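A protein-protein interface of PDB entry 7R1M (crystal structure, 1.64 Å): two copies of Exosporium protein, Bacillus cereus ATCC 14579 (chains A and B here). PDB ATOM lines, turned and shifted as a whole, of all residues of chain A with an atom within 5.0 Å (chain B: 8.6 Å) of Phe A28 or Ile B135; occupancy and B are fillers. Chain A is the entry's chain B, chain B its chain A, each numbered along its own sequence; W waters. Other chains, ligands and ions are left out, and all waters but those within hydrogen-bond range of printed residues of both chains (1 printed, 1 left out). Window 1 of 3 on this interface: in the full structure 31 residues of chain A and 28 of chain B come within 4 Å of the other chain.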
ATOM      1  N   PHE A  26     -29.904   8.926 -20.591  1.00  0.00           N
ATOM      2  CA  PHE A  26     -28.778   9.527 -21.361  1.00  0.00           C
ATOM      3  C   PHE A  26     -28.345   8.565 -22.451  1.00  0.00           C
ATOM      4  O   PHE A  26     -28.702   7.375 -22.398  1.00  0.00           O
ATOM      5  CB  PHE A  26     -27.617   9.936 -20.436  1.00  0.00           C
ATOM      6  CG  PHE A  26     -27.027   8.821 -19.601  1.00  0.00           C
ATOM      7  CD1 PHE A  26     -26.155   7.902 -20.156  1.00  0.00           C
ATOM      8  CD2 PHE A  26     -27.370   8.683 -18.260  1.00  0.00           C
ATOM      9  CE1 PHE A  26     -25.584   6.912 -19.373  1.00  0.00           C
ATOM     10  CE2 PHE A  26     -26.807   7.682 -17.482  1.00  0.00           C
ATOM     11  CZ  PHE A  26     -25.931   6.795 -18.043  1.00  0.00           C
ATOM     12  N   GLY A  27     -27.644   9.103 -23.459  1.00  0.00           N
ATOM     13  CA  GLY A  27     -27.019   8.285 -24.500  1.00  0.00           C
ATOM     14  C   GLY A  27     -25.883   9.072 -25.132  1.00  0.00           C
ATOM     15  O   GLY A  27     -26.027  10.293 -25.259  1.00  0.00           O
ATOM     16  N   PHE A  28     -24.832   8.370 -25.531  1.00  0.00           N
ATOM     17  CA  PHE A  28     -23.689   8.909 -26.307  1.00  0.00           C
ATOM     18  C   PHE A  28     -23.469   7.961 -27.470  1.00  0.00           C
ATOM     19  O   PHE A  28     -23.196   6.789 -27.245  1.00  0.00           O
ATOM     20  CB  PHE A  28     -22.474   9.113 -25.422  1.00  0.00           C
ATOM     21  CG  PHE A  28     -21.340   9.803 -26.129  1.00  0.00           C
ATOM     22  CD1 PHE A  28     -21.378  11.168 -26.345  1.00  0.00           C
ATOM     23  CD2 PHE A  28     -20.236   9.089 -26.580  1.00  0.00           C
ATOM     24  CE1 PHE A  28     -20.334  11.806 -26.997  1.00  0.00           C
ATOM     25  CE2 PHE A  28     -19.196   9.729 -27.225  1.00  0.00           C
ATOM     26  CZ  PHE A  28     -19.245  11.084 -27.442  1.00  0.00           C
ATOM     27  N   ALA A  29     -23.724   8.438 -28.683  1.00  0.00           N
ATOM     28  CA  ALA A  29     -23.586   7.645 -29.919  1.00  0.00           C
ATOM     29  C   ALA A  29     -22.565   8.368 -30.788  1.00  0.00           C
ATOM     30  O   ALA A  29     -22.681   9.612 -30.945  1.00  0.00           O
ATOM     31  CB  ALA A  29     -24.898   7.446 -30.628  1.00  0.00           C
ATOM     32  N   PHE A  30     -21.542   7.655 -31.228  1.00  0.00           N
ATOM     33  CA  PHE A  30     -20.437   8.282 -31.987  1.00  0.00           C
ATOM     34  C   PHE A  30     -19.927   7.349 -33.075  1.00  0.00           C
ATOM     35  O   PHE A  30     -20.237   6.145 -33.091  1.00  0.00           O
ATOM     36  CB  PHE A  30     -19.336   8.733 -31.017  1.00  0.00           C
ATOM     37  CG  PHE A  30     -18.535   7.619 -30.400  1.00  0.00           C
ATOM     38  CD1 PHE A  30     -19.007   6.930 -29.285  1.00  0.00           C
ATOM     39  CD2 PHE A  30     -17.331   7.224 -30.958  1.00  0.00           C
ATOM     40  CE1 PHE A  30     -18.268   5.906 -28.716  1.00  0.00           C
ATOM     41  CE2 PHE A  30     -16.582   6.212 -30.376  1.00  0.00           C
ATOM     42  CZ  PHE A  30     -17.062   5.537 -29.268  1.00  0.00           C
ATOM     43  N   SER A  48     -21.267   3.509 -32.519  1.00  0.00           N
ATOM     44  CA  SER A  48     -20.627   3.165 -31.230  1.00  0.00           C
ATOM     45  C   SER A  48     -21.326   3.893 -30.083  1.00  0.00           C
ATOM     46  O   SER A  48     -21.832   5.040 -30.262  1.00  0.00           O
ATOM     47  CB  SER A  48     -19.161   3.453 -31.218  1.00  0.00           C
ATOM     48  OG  SER A  48     -18.551   2.955 -32.400  1.00  0.00           O
ATOM     49  N   VAL A  49     -21.278   3.274 -28.906  1.00  0.00           N
ATOM     50  CA  VAL A  49     -21.845   3.846 -27.654  1.00  0.00           C
ATOM     51  C   VAL A  49     -20.877   3.734 -26.490  1.00  0.00           C
ATOM     52  O   VAL A  49     -21.309   4.080 -25.355  1.00  0.00           O
ATOM     53  CB  VAL A  49     -23.168   3.143 -27.328  1.00  0.00           C
ATOM     54  CG1 VAL A  49     -24.180   3.407 -28.410  1.00  0.00           C
ATOM     55  CG2 VAL A  49     -22.960   1.650 -27.098  1.00  0.00           C
ATOM     56  N   PRO A  51     -17.344   5.058 -25.320  1.00  0.00           N
ATOM     57  CA  PRO A  51     -16.179   5.919 -25.555  1.00  0.00           C
ATOM     58  C   PRO A  51     -14.949   5.693 -24.663  1.00  0.00           C
ATOM     59  O   PRO A  51     -13.902   6.121 -25.059  1.00  0.00           O
ATOM     60  CB  PRO A  51     -16.730   7.337 -25.291  1.00  0.00           C
ATOM     61  CG  PRO A  51     -17.851   7.110 -24.278  1.00  0.00           C
ATOM     62  CD  PRO A  51     -18.455   5.771 -24.672  1.00  0.00           C
ATOM     63  N   VAL A  59     -22.598   3.738 -22.858  1.00  0.00           N
ATOM     64  CA  VAL A  59     -23.009   4.970 -22.147  1.00  0.00           C
ATOM     65  C   VAL A  59     -24.426   5.286 -22.621  1.00  0.00           C
ATOM     66  O   VAL A  59     -24.662   6.218 -23.445  1.00  0.00           O
ATOM     67  CB  VAL A  59     -21.976   6.104 -22.334  1.00  0.00           C
ATOM     68  CG1 VAL A  59     -22.446   7.390 -21.673  1.00  0.00           C
ATOM     69  CG2 VAL A  59     -20.626   5.726 -21.738  1.00  0.00           C
ATOM     70  N   ILE A  60     -25.361   4.486 -22.118  1.00  0.00           N
ATOM     71  CA  ILE A  60     -26.766   4.392 -22.594  1.00  0.00           C
ATOM     72  C   ILE A  60     -27.560   4.034 -21.353  1.00  0.00           C
ATOM     73  O   ILE A  60     -27.207   3.023 -20.734  1.00  0.00           O
ATOM     74  CB  ILE A  60     -26.938   3.330 -23.699  1.00  0.00           C
ATOM     75  CG1 ILE A  60     -26.148   3.665 -24.968  1.00  0.00           C
ATOM     76  CG2 ILE A  60     -28.417   3.106 -24.008  1.00  0.00           C
ATOM     77  CD1 ILE A  60     -26.784   4.762 -25.802  1.00  0.00           C
ATOM     78  N   ILE A  70     -30.364   8.815 -31.622  1.00  0.00           N
ATOM     79  CA  ILE A  70     -30.773   8.336 -30.282  1.00  0.00           C
ATOM     80  C   ILE A  70     -32.292   8.499 -30.156  1.00  0.00           C
ATOM     81  O   ILE A  70     -32.852   9.585 -30.512  1.00  0.00           O
ATOM     82  CB  ILE A  70     -29.958   9.054 -29.203  1.00  0.00           C
ATOM     83  CG1 ILE A  70     -28.515   8.538 -29.219  1.00  0.00           C
ATOM     84  CG2 ILE A  70     -30.594   8.894 -27.832  1.00  0.00           C
ATOM     85  CD1 ILE A  70     -27.575   9.377 -28.424  1.00  0.00           C
ATOM     86  N   ALA A 162     -20.347  12.632 -33.259  1.00  0.00           N
ATOM     87  CA  ALA A 162     -20.769  12.209 -31.917  1.00  0.00           C
ATOM     88  C   ALA A 162     -21.993  13.007 -31.519  1.00  0.00           C
ATOM     89  O   ALA A 162     -22.019  14.211 -31.755  1.00  0.00           O
ATOM     90  CB  ALA A 162     -19.657  12.412 -30.943  1.00  0.00           C
ATOM     91  N   LEU A 163     -22.970  12.313 -30.974  1.00  0.00           N
ATOM     92  CA  LEU A 163     -24.254  12.890 -30.515  1.00  0.00           C
ATOM     93  C   LEU A 163     -24.393  12.609 -29.014  1.00  0.00           C
ATOM     94  O   LEU A 163     -24.174  11.468 -28.591  1.00  0.00           O
ATOM     95  CB  LEU A 163     -25.383  12.251 -31.326  1.00  0.00           C
ATOM     96  CG  LEU A 163     -26.810  12.599 -30.902  1.00  0.00           C
ATOM     97  CD1 LEU A 163     -27.114  14.057 -31.098  1.00  0.00           C
ATOM     98  CD2 LEU A 163     -27.809  11.749 -31.675  1.00  0.00           C
ATOM     99  N   THR A 164     -24.773  13.630 -28.266  1.00  0.00           N
ATOM    100  CA  THR A 164     -24.854  13.638 -26.798  1.00  0.00           C
ATOM    101  C   THR A 164     -26.285  13.992 -26.417  1.00  0.00           C
ATOM    102  O   THR A 164     -26.718  15.049 -26.803  1.00  0.00           O
ATOM    103  CB  THR A 164     -23.854  14.613 -26.169  1.00  0.00           C
ATOM    104  OG1 THR A 164     -22.538  14.232 -26.581  1.00  0.00           O
ATOM    105  CG2 THR A 164     -23.980  14.635 -24.661  1.00  0.00           C
ATOM    106  N   ILE B  77     -21.244   8.513 -14.350  1.00  0.00           N
ATOM    107  CA  ILE B  77     -21.243   8.952 -15.774  1.00  0.00           C
ATOM    108  C   ILE B  77     -20.982  10.456 -15.749  1.00  0.00           C
ATOM    109  O   ILE B  77     -21.643  11.145 -14.956  1.00  0.00           O
ATOM    110  CB  ILE B  77     -22.579   8.601 -16.456  1.00  0.00           C
ATOM    111  CG1 ILE B  77     -22.886   7.107 -16.340  1.00  0.00           C
ATOM    112  CG2 ILE B  77     -22.590   9.069 -17.903  1.00  0.00           C
ATOM    113  CD1 ILE B  77     -21.937   6.228 -17.117  1.00  0.00           C
ATOM    114  N   TYR B  78     -20.037  10.937 -16.555  1.00  0.00           N
ATOM    115  CA  TYR B  78     -19.668  12.369 -16.463  1.00  0.00           C
ATOM    116  C   TYR B  78     -19.660  13.062 -17.820  1.00  0.00           C
ATOM    117  O   TYR B  78     -19.247  12.432 -18.806  1.00  0.00           O
ATOM    118  CB  TYR B  78     -18.234  12.515 -15.949  1.00  0.00           C
ATOM    119  CG  TYR B  78     -18.035  12.323 -14.467  1.00  0.00           C
ATOM    120  CD1 TYR B  78     -17.987  11.059 -13.907  1.00  0.00           C
ATOM    121  CD2 TYR B  78     -17.861  13.410 -13.628  1.00  0.00           C
ATOM    122  CE1 TYR B  78     -17.796  10.879 -12.548  1.00  0.00           C
ATOM    123  CE2 TYR B  78     -17.666  13.249 -12.268  1.00  0.00           C
ATOM    124  CZ  TYR B  78     -17.635  11.978 -11.725  1.00  0.00           C
ATOM    125  OH  TYR B  78     -17.446  11.811 -10.386  1.00  0.00           O
ATOM    126  N   GLN B  79     -20.133  14.307 -17.868  1.00  0.00           N
ATOM    127  CA  GLN B  79     -19.982  15.128 -19.081  1.00  0.00           C
ATOM    128  C   GLN B  79     -18.622  15.809 -18.961  1.00  0.00           C
ATOM    129  O   GLN B  79     -18.320  16.349 -17.919  1.00  0.00           O
ATOM    130  CB  GLN B  79     -21.145  16.102 -19.257  1.00  0.00           C
ATOM    131  CG  GLN B  79     -21.290  17.130 -18.165  1.00  0.00           C
ATOM    132  CD  GLN B  79     -22.160  18.263 -18.653  1.00  0.00           C
ATOM    133  OE1 GLN B  79     -23.360  18.307 -18.401  1.00  0.00           O
ATOM    134  NE2 GLN B  79     -21.562  19.166 -19.418  1.00  0.00           N
ATOM    135  N   ILE B  80     -17.828  15.742 -20.009  1.00  0.00           N
ATOM    136  CA  ILE B  80     -16.499  16.423 -20.056  1.00  0.00           C
ATOM    137  C   ILE B  80     -16.426  17.227 -21.359  1.00  0.00           C
ATOM    138  O   ILE B  80     -16.965  16.798 -22.421  1.00  0.00           O
ATOM    139  CB  ILE B  80     -15.350  15.394 -19.920  1.00  0.00           C
ATOM    140  CG1 ILE B  80     -15.278  14.431 -21.097  1.00  0.00           C
ATOM    141  CG2 ILE B  80     -15.478  14.623 -18.597  1.00  0.00           C
ATOM    142  CD1 ILE B  80     -14.144  13.456 -20.986  1.00  0.00           C
ATOM    143  N   SER B  81     -15.777  18.359 -21.304  1.00  0.00           N
ATOM    144  CA  SER B  81     -15.649  19.280 -22.454  1.00  0.00           C
ATOM    145  C   SER B  81     -14.600  20.324 -22.140  1.00  0.00           C
ATOM    146  O   SER B  81     -14.170  20.466 -20.956  1.00  0.00           O
ATOM    147  CB  SER B  81     -17.004  19.918 -22.772  1.00  0.00           C
ATOM    148  OG  SER B  81     -17.419  20.758 -21.718  1.00  0.00           O
ATOM    149  N   TYR B  82     -14.109  21.009 -23.173  1.00  0.00           N
ATOM    150  CA  TYR B  82     -13.068  22.033 -22.982  1.00  0.00           C
ATOM    151  C   TYR B  82     -13.137  23.075 -24.093  1.00  0.00           C
ATOM    152  O   TYR B  82     -13.778  22.842 -25.109  1.00  0.00           O
ATOM    153  CB  TYR B  82     -11.679  21.400 -22.897  1.00  0.00           C
ATOM    154  CG  TYR B  82     -11.165  20.857 -24.198  1.00  0.00           C
ATOM    155  CD1 TYR B  82     -11.573  19.620 -24.652  1.00  0.00           C
ATOM    156  CD2 TYR B  82     -10.343  21.601 -25.015  1.00  0.00           C
ATOM    157  CE1 TYR B  82     -11.143  19.131 -25.864  1.00  0.00           C
ATOM    158  CE2 TYR B  82      -9.925  21.127 -26.238  1.00  0.00           C
ATOM    159  CZ  TYR B  82     -10.308  19.876 -26.657  1.00  0.00           C
ATOM    160  OH  TYR B  82      -9.884  19.358 -27.849  1.00  0.00           O
ATOM    161  N   PHE B 101      -7.178  17.050 -28.087  1.00  0.00           N
ATOM    162  CA  PHE B 101      -8.155  16.066 -27.579  1.00  0.00           C
ATOM    163  C   PHE B 101      -8.128  16.111 -26.056  1.00  0.00           C
ATOM    164  O   PHE B 101      -7.182  16.639 -25.454  1.00  0.00           O
ATOM    165  CB  PHE B 101      -7.857  14.619 -28.007  1.00  0.00           C
ATOM    166  CG  PHE B 101      -8.254  14.294 -29.429  1.00  0.00           C
ATOM    167  CD1 PHE B 101      -7.406  14.594 -30.485  1.00  0.00           C
ATOM    168  CD2 PHE B 101      -9.497  13.756 -29.729  1.00  0.00           C
ATOM    169  CE1 PHE B 101      -7.807  14.376 -31.798  1.00  0.00           C
ATOM    170  CE2 PHE B 101      -9.869  13.479 -31.036  1.00  0.00           C
ATOM    171  CZ  PHE B 101      -9.037  13.820 -32.067  1.00  0.00           C
ATOM    172  N   LEU B 102      -9.114  15.440 -25.466  1.00  0.00           N
ATOM    173  CA  LEU B 102      -9.076  15.188 -24.015  1.00  0.00           C
ATOM    174  C   LEU B 102      -8.442  13.799 -23.855  1.00  0.00           C
ATOM    175  O   LEU B 102      -8.675  12.951 -24.721  1.00  0.00           O
ATOM    176  CB  LEU B 102     -10.498  15.173 -23.461  1.00  0.00           C
ATOM    177  CG  LEU B 102     -11.133  16.543 -23.269  1.00  0.00           C
ATOM    178  CD1 LEU B 102     -12.574  16.416 -22.813  1.00  0.00           C
ATOM    179  CD2 LEU B 102     -10.322  17.365 -22.287  1.00  0.00           C
ATOM    180  N   ILE B 111      -9.765  10.517 -26.050  1.00  0.00           N
ATOM    181  CA  ILE B 111     -11.196  10.154 -25.914  1.00  0.00           C
ATOM    182  C   ILE B 111     -11.914  10.560 -27.189  1.00  0.00           C
ATOM    183  O   ILE B 111     -11.888  11.728 -27.556  1.00  0.00           O
ATOM    184  CB  ILE B 111     -11.791  10.834 -24.683  1.00  0.00           C
ATOM    185  CG1 ILE B 111     -11.041  10.401 -23.424  1.00  0.00           C
ATOM    186  CG2 ILE B 111     -13.291  10.540 -24.571  1.00  0.00           C
ATOM    187  CD1 ILE B 111     -11.295  11.253 -22.220  1.00  0.00           C
ATOM    188  N   PRO B 112     -12.657   9.637 -27.823  1.00  0.00           N
ATOM    189  CA  PRO B 112     -13.370   9.955 -29.058  1.00  0.00           C
ATOM    190  C   PRO B 112     -14.403  11.059 -28.807  1.00  0.00           C
ATOM    191  O   PRO B 112     -14.950  11.134 -27.730  1.00  0.00           O
ATOM    192  CB  PRO B 112     -14.000   8.620 -29.478  1.00  0.00           C
ATOM    193  CG  PRO B 112     -14.012   7.794 -28.216  1.00  0.00           C
ATOM    194  CD  PRO B 112     -12.767   8.210 -27.444  1.00  0.00           C
ATOM    195  N   GLY B 113     -14.594  11.911 -29.800  1.00  0.00           N
ATOM    196  CA  GLY B 113     -15.525  13.037 -29.782  1.00  0.00           C
ATOM    197  C   GLY B 113     -14.942  14.342 -29.250  1.00  0.00           C
ATOM    198  O   GLY B 113     -15.700  15.310 -29.217  1.00  0.00           O
ATOM    199  N   SER B 114     -13.705  14.361 -28.731  1.00  0.00           N
ATOM    200  CA  SER B 114     -13.162  15.509 -27.970  1.00  0.00           C
ATOM    201  C   SER B 114     -12.195  16.324 -28.831  1.00  0.00           C
ATOM    202  O   SER B 114     -11.432  17.112 -28.266  1.00  0.00           O
ATOM    203  CB  SER B 114     -12.510  15.017 -26.681  1.00  0.00           C
ATOM    204  OG  SER B 114     -11.388  14.182 -26.930  1.00  0.00           O
ATOM    205  N   GLY B 115     -12.158  16.122 -30.158  1.00  0.00           N
ATOM    206  CA  GLY B 115     -11.227  16.869 -31.034  1.00  0.00           C
ATOM    207  C   GLY B 115     -11.561  18.353 -31.118  1.00  0.00           C
ATOM    208  O   GLY B 115     -12.763  18.721 -31.226  1.00  0.00           O
ATOM    209  N   SER B 132     -14.810  22.120 -27.731  1.00  0.00           N
ATOM    210  CA  SER B 132     -15.111  20.701 -27.981  1.00  0.00           C
ATOM    211  C   SER B 132     -16.613  20.507 -27.851  1.00  0.00           C
ATOM    212  O   SER B 132     -17.349  21.460 -27.462  1.00  0.00           O
ATOM    213  CB  SER B 132     -14.392  19.814 -27.002  1.00  0.00           C
ATOM    214  OG  SER B 132     -15.014  19.887 -25.718  1.00  0.00           O
ATOM    215  N   GLY B 133     -17.050  19.332 -28.211  1.00  0.00           N
ATOM    216  CA  GLY B 133     -18.382  18.875 -27.804  1.00  0.00           C
ATOM    217  C   GLY B 133     -18.378  18.423 -26.371  1.00  0.00           C
ATOM    218  O   GLY B 133     -17.312  18.489 -25.701  1.00  0.00           O
ATOM    219  N   VAL B 134     -19.527  17.919 -25.966  1.00  0.00           N
ATOM    220  CA  VAL B 134     -19.753  17.386 -24.604  1.00  0.00           C
ATOM    221  C   VAL B 134     -19.721  15.870 -24.725  1.00  0.00           C
ATOM    222  O   VAL B 134     -20.504  15.311 -25.475  1.00  0.00           O
ATOM    223  CB  VAL B 134     -21.067  17.930 -24.016  1.00  0.00           C
ATOM    224  CG1 VAL B 134     -21.248  17.383 -22.602  1.00  0.00           C
ATOM    225  CG2 VAL B 134     -21.097  19.434 -24.001  1.00  0.00           C
ATOM    226  N   ILE B 135     -18.727  15.251 -24.116  1.00  0.00           N
ATOM    227  CA  ILE B 135     -18.594  13.776 -24.124  1.00  0.00           C
ATOM    228  C   ILE B 135     -19.250  13.237 -22.851  1.00  0.00           C
ATOM    229  O   ILE B 135     -18.970  13.782 -21.805  1.00  0.00           O
ATOM    230  CB  ILE B 135     -17.102  13.403 -24.184  1.00  0.00           C
ATOM    231  CG1 ILE B 135     -16.368  14.104 -25.329  1.00  0.00           C
ATOM    232  CG2 ILE B 135     -16.969  11.905 -24.249  1.00  0.00           C
ATOM    233  CD1 ILE B 135     -16.967  13.813 -26.655  1.00  0.00           C
ATOM    234  N   LEU B 136     -20.032  12.170 -22.950  1.00  0.00           N
ATOM    235  CA  LEU B 136     -20.553  11.421 -21.774  1.00  0.00           C
ATOM    236  C   LEU B 136     -19.705  10.163 -21.655  1.00  0.00           C
ATOM    237  O   LEU B 136     -19.521   9.477 -22.678  1.00  0.00           O
ATOM    238  CB  LEU B 136     -22.017  11.027 -21.929  1.00  0.00           C
ATOM    239  CG  LEU B 136     -23.006  12.155 -22.188  1.00  0.00           C
ATOM    240  CD1 LEU B 136     -24.426  11.611 -22.171  1.00  0.00           C
ATOM    241  CD2 LEU B 136     -22.839  13.288 -21.209  1.00  0.00           C
ATOM    242  N   ILE B 137     -19.143   9.974 -20.470  1.00  0.00           N
ATOM    243  CA  ILE B 137     -18.190   8.862 -20.251  1.00  0.00           C
ATOM    244  C   ILE B 137     -18.236   8.366 -18.804  1.00  0.00           C
ATOM    245  O   ILE B 137     -18.414   9.148 -17.901  1.00  0.00           O
ATOM    246  CB  ILE B 137     -16.780   9.344 -20.638  1.00  0.00           C
ATOM    247  CG1 ILE B 137     -15.727   8.250 -20.495  1.00  0.00           C
ATOM    248  CG2 ILE B 137     -16.400  10.577 -19.862  1.00  0.00           C
ATOM    249  CD1 ILE B 137     -14.490   8.484 -21.282  1.00  0.00           C
ATOM    250  N   ASN B 138     -18.114   7.061 -18.655  1.00  0.00           N
ATOM    251  CA  ASN B 138     -18.002   6.412 -17.337  1.00  0.00           C
ATOM    252  C   ASN B 138     -16.582   6.666 -16.832  1.00  0.00           C
ATOM    253  O   ASN B 138     -15.661   6.377 -17.559  1.00  0.00           O
ATOM    254  CB  ASN B 138     -18.258   4.914 -17.467  1.00  0.00           C
ATOM    255  CG  ASN B 138     -17.420   4.249 -18.535  1.00  0.00           C
ATOM    256  OD1 ASN B 138     -17.524   4.563 -19.701  1.00  0.00           O
ATOM    257  ND2 ASN B 138     -16.599   3.304 -18.140  1.00  0.00           N
ATOM    258  N   LEU B 139     -16.451   7.227 -15.628  1.00  0.00           N
ATOM    259  CA  LEU B 139     -15.116   7.486 -15.031  1.00  0.00           C
ATOM    260  C   LEU B 139     -15.053   6.816 -13.658  1.00  0.00           C
ATOM    261  O   LEU B 139     -16.117   6.597 -13.057  1.00  0.00           O
ATOM    262  CB  LEU B 139     -14.866   8.993 -14.933  1.00  0.00           C
ATOM    263  CG  LEU B 139     -14.760   9.729 -16.266  1.00  0.00           C
ATOM    264  CD1 LEU B 139     -14.523  11.212 -16.046  1.00  0.00           C
ATOM    265  CD2 LEU B 139     -13.660   9.135 -17.130  1.00  0.00           C
ATOM    266  N   ILE B 145      -8.411  13.639 -16.146  1.00  0.00           N
ATOM    267  CA  ILE B 145      -8.837  14.210 -17.449  1.00  0.00           C
ATOM    268  C   ILE B 145      -7.941  15.410 -17.758  1.00  0.00           C
ATOM    269  O   ILE B 145      -7.795  16.260 -16.895  1.00  0.00           O
ATOM    270  CB  ILE B 145     -10.335  14.563 -17.445  1.00  0.00           C
ATOM    271  CG1 ILE B 145     -11.192  13.378 -16.996  1.00  0.00           C
ATOM    272  CG2 ILE B 145     -10.766  15.090 -18.804  1.00  0.00           C
ATOM    273  CD1 ILE B 145     -11.180  12.221 -17.958  1.00  0.00           C
ATOM    274  N   THR B 164     -14.090  21.374 -18.261  1.00  0.00           N
ATOM    275  CA  THR B 164     -15.362  21.235 -17.538  1.00  0.00           C
ATOM    276  C   THR B 164     -15.611  19.745 -17.294  1.00  0.00           C
ATOM    277  O   THR B 164     -15.652  18.966 -18.250  1.00  0.00           O
ATOM    278  CB  THR B 164     -16.500  21.855 -18.362  1.00  0.00           C
ATOM    279  OG1 THR B 164     -16.155  23.220 -18.573  1.00  0.00           O
ATOM    280  CG2 THR B 164     -17.840  21.722 -17.673  1.00  0.00           C
ATOM    281  N   VAL B 165     -15.834  19.362 -16.031  1.00  0.00           N
ATOM    282  CA  VAL B 165     -16.187  17.983 -15.649  1.00  0.00           C
ATOM    283  C   VAL B 165     -17.405  18.077 -14.730  1.00  0.00           C
ATOM    284  O   VAL B 165     -17.286  18.817 -13.746  1.00  0.00           O
ATOM    285  CB  VAL B 165     -14.995  17.309 -14.958  1.00  0.00           C
ATOM    286  CG1 VAL B 165     -15.398  15.954 -14.416  1.00  0.00           C
ATOM    287  CG2 VAL B 165     -13.830  17.171 -15.919  1.00  0.00           C
ATOM    288  N   ALA B 166     -18.507  17.393 -15.061  1.00  0.00           N
ATOM    289  CA  ALA B 166     -19.724  17.392 -14.213  1.00  0.00           C
ATOM    290  C   ALA B 166     -20.361  15.999 -14.229  1.00  0.00           C
ATOM    291  O   ALA B 166     -20.435  15.407 -15.315  1.00  0.00           O
ATOM    292  CB  ALA B 166     -20.691  18.451 -14.678  1.00  0.00           C
ATOM    293  N   ILE B 168     -23.131  13.437 -14.558  1.00  0.00           N
ATOM    294  CA  ILE B 168     -24.541  13.260 -15.016  1.00  0.00           C
ATOM    295  C   ILE B 168     -25.271  12.281 -14.091  1.00  0.00           C
ATOM    296  O   ILE B 168     -26.412  12.581 -13.701  1.00  0.00           O
ATOM    297  CB  ILE B 168     -24.557  12.774 -16.480  1.00  0.00           C
ATOM    298  CG1 ILE B 168     -23.884  13.785 -17.410  1.00  0.00           C
ATOM    299  CG2 ILE B 168     -25.968  12.446 -16.938  1.00  0.00           C
ATOM    300  CD1 ILE B 168     -24.572  15.128 -17.441  1.00  0.00           C
HETATM  301  O   HOH W   1     -21.292  15.177 -28.782  1.00  0.00           O
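The side-chain hydroxyl (OG1) of Thr A164 lies within hydrogen-bond range of the backbone carbonyl oxygen (O) of Val B134 (2.6 Å).
Of chain B, only Val B134, Ile B135 and Leu B136 come within 4 Å of Phe A28. No residue of chain B comes within 4 Å of Ala A29. Of the printed residues of chain B, Val A59 touches Leu B136 (3.7 Å) and Asn B138 (3.9 Å). Ala A162 touches none of the printed residues of chain B. Printed residues of chain A within 4 Å of Ile B77: Phe A26 (3.5 Å). Printed residues of chain A within 4 Å of Pro B112: Phe A30 and Pro A51. Gly B113 touches none of the printed residues of chain A. Ile B135 touches just one residue of chain A: Phe A28. Printed residues of chain A within 4 Å of Leu B136: Phe A26, Gly A27, Phe A28, Pro A51, Val A59 and Thr A164. Of the printed residues of chain A, Asn B138 touches Val A59. The nearest residue of chain B that does not touch Phe A28 is Pro B112 (4.3 Å). The nearest printed residue of chain B that does not touch Phe A26 is Ile B168 (4.2 Å).
The backbone carbonyl oxygen of Ile B77 sits at hydrogen-bond distance from the backbone NH of Ile B168, at 2.8 Å. O of Ile B80 is in hydrogen-bond range of N of Ile B135, at 2.9 Å. The backbone NH (N) of Phe A28 is in hydrogen-bond range of the backbone carbonyl oxygen (O) of Val A59, at 3.0 Å. N of Phe A30 sits at hydrogen-bond distance from O of Ser A48 (2.8 Å). The backbone NH (N) of Val A59 sits at hydrogen-bond distance from the backbone carbonyl oxygen (O) of Val A49 (2.8 Å).
Position printed for both chains: 164.
Among the printed residues, merely in contact across the chains: Phe A26 with Ile B77 (3.5 Å), Phe A26 with Leu B136 (3.9998 Å), Gly A27 with Leu B136 (3.7 Å), Phe A28 with Val B134 (3.8 Å), Phe A28 with Ile B135 (3.6 Å), Phe A28 with Leu B136 (3.8 Å), Phe A30 with Pro B112 (3.6 Å), Pro A51 with Pro B112 (3.4 Å), Pro A51 with Leu B136 (3.3 Å), Val A59 with Leu B136 (3.7 Å), Val A59 with Asn B138 (3.9 Å) and Thr A164 with Leu B136 (3.6 Å).
Water W1 lies within hydrogen-bond range of OG1 of Thr A164 (2.7 Å), O of Ala A162 (3.2 Å) and O of Val B134 (3.4 Å).
Hydrophobic or aromatic side chains of chain B within 4 Å of the printed part of chain A: Ile B77, Pro B112, Ile B135 and Leu B136. Hydrophobic or aromatic side chains of chain A that line the printed part of chain B: Phe A26, Phe A28, Phe A30, Pro A51 and Val A59. Along chain A the printed residues that touch a printed residue of chain B span positions 26 to 164. Among the printed residues, 13 pairs touch across the chains. Among the printed residues, no Asp or Glu carboxylate lies within 4 Å of a Lys or Arg side-chain nitrogen of the other chain.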
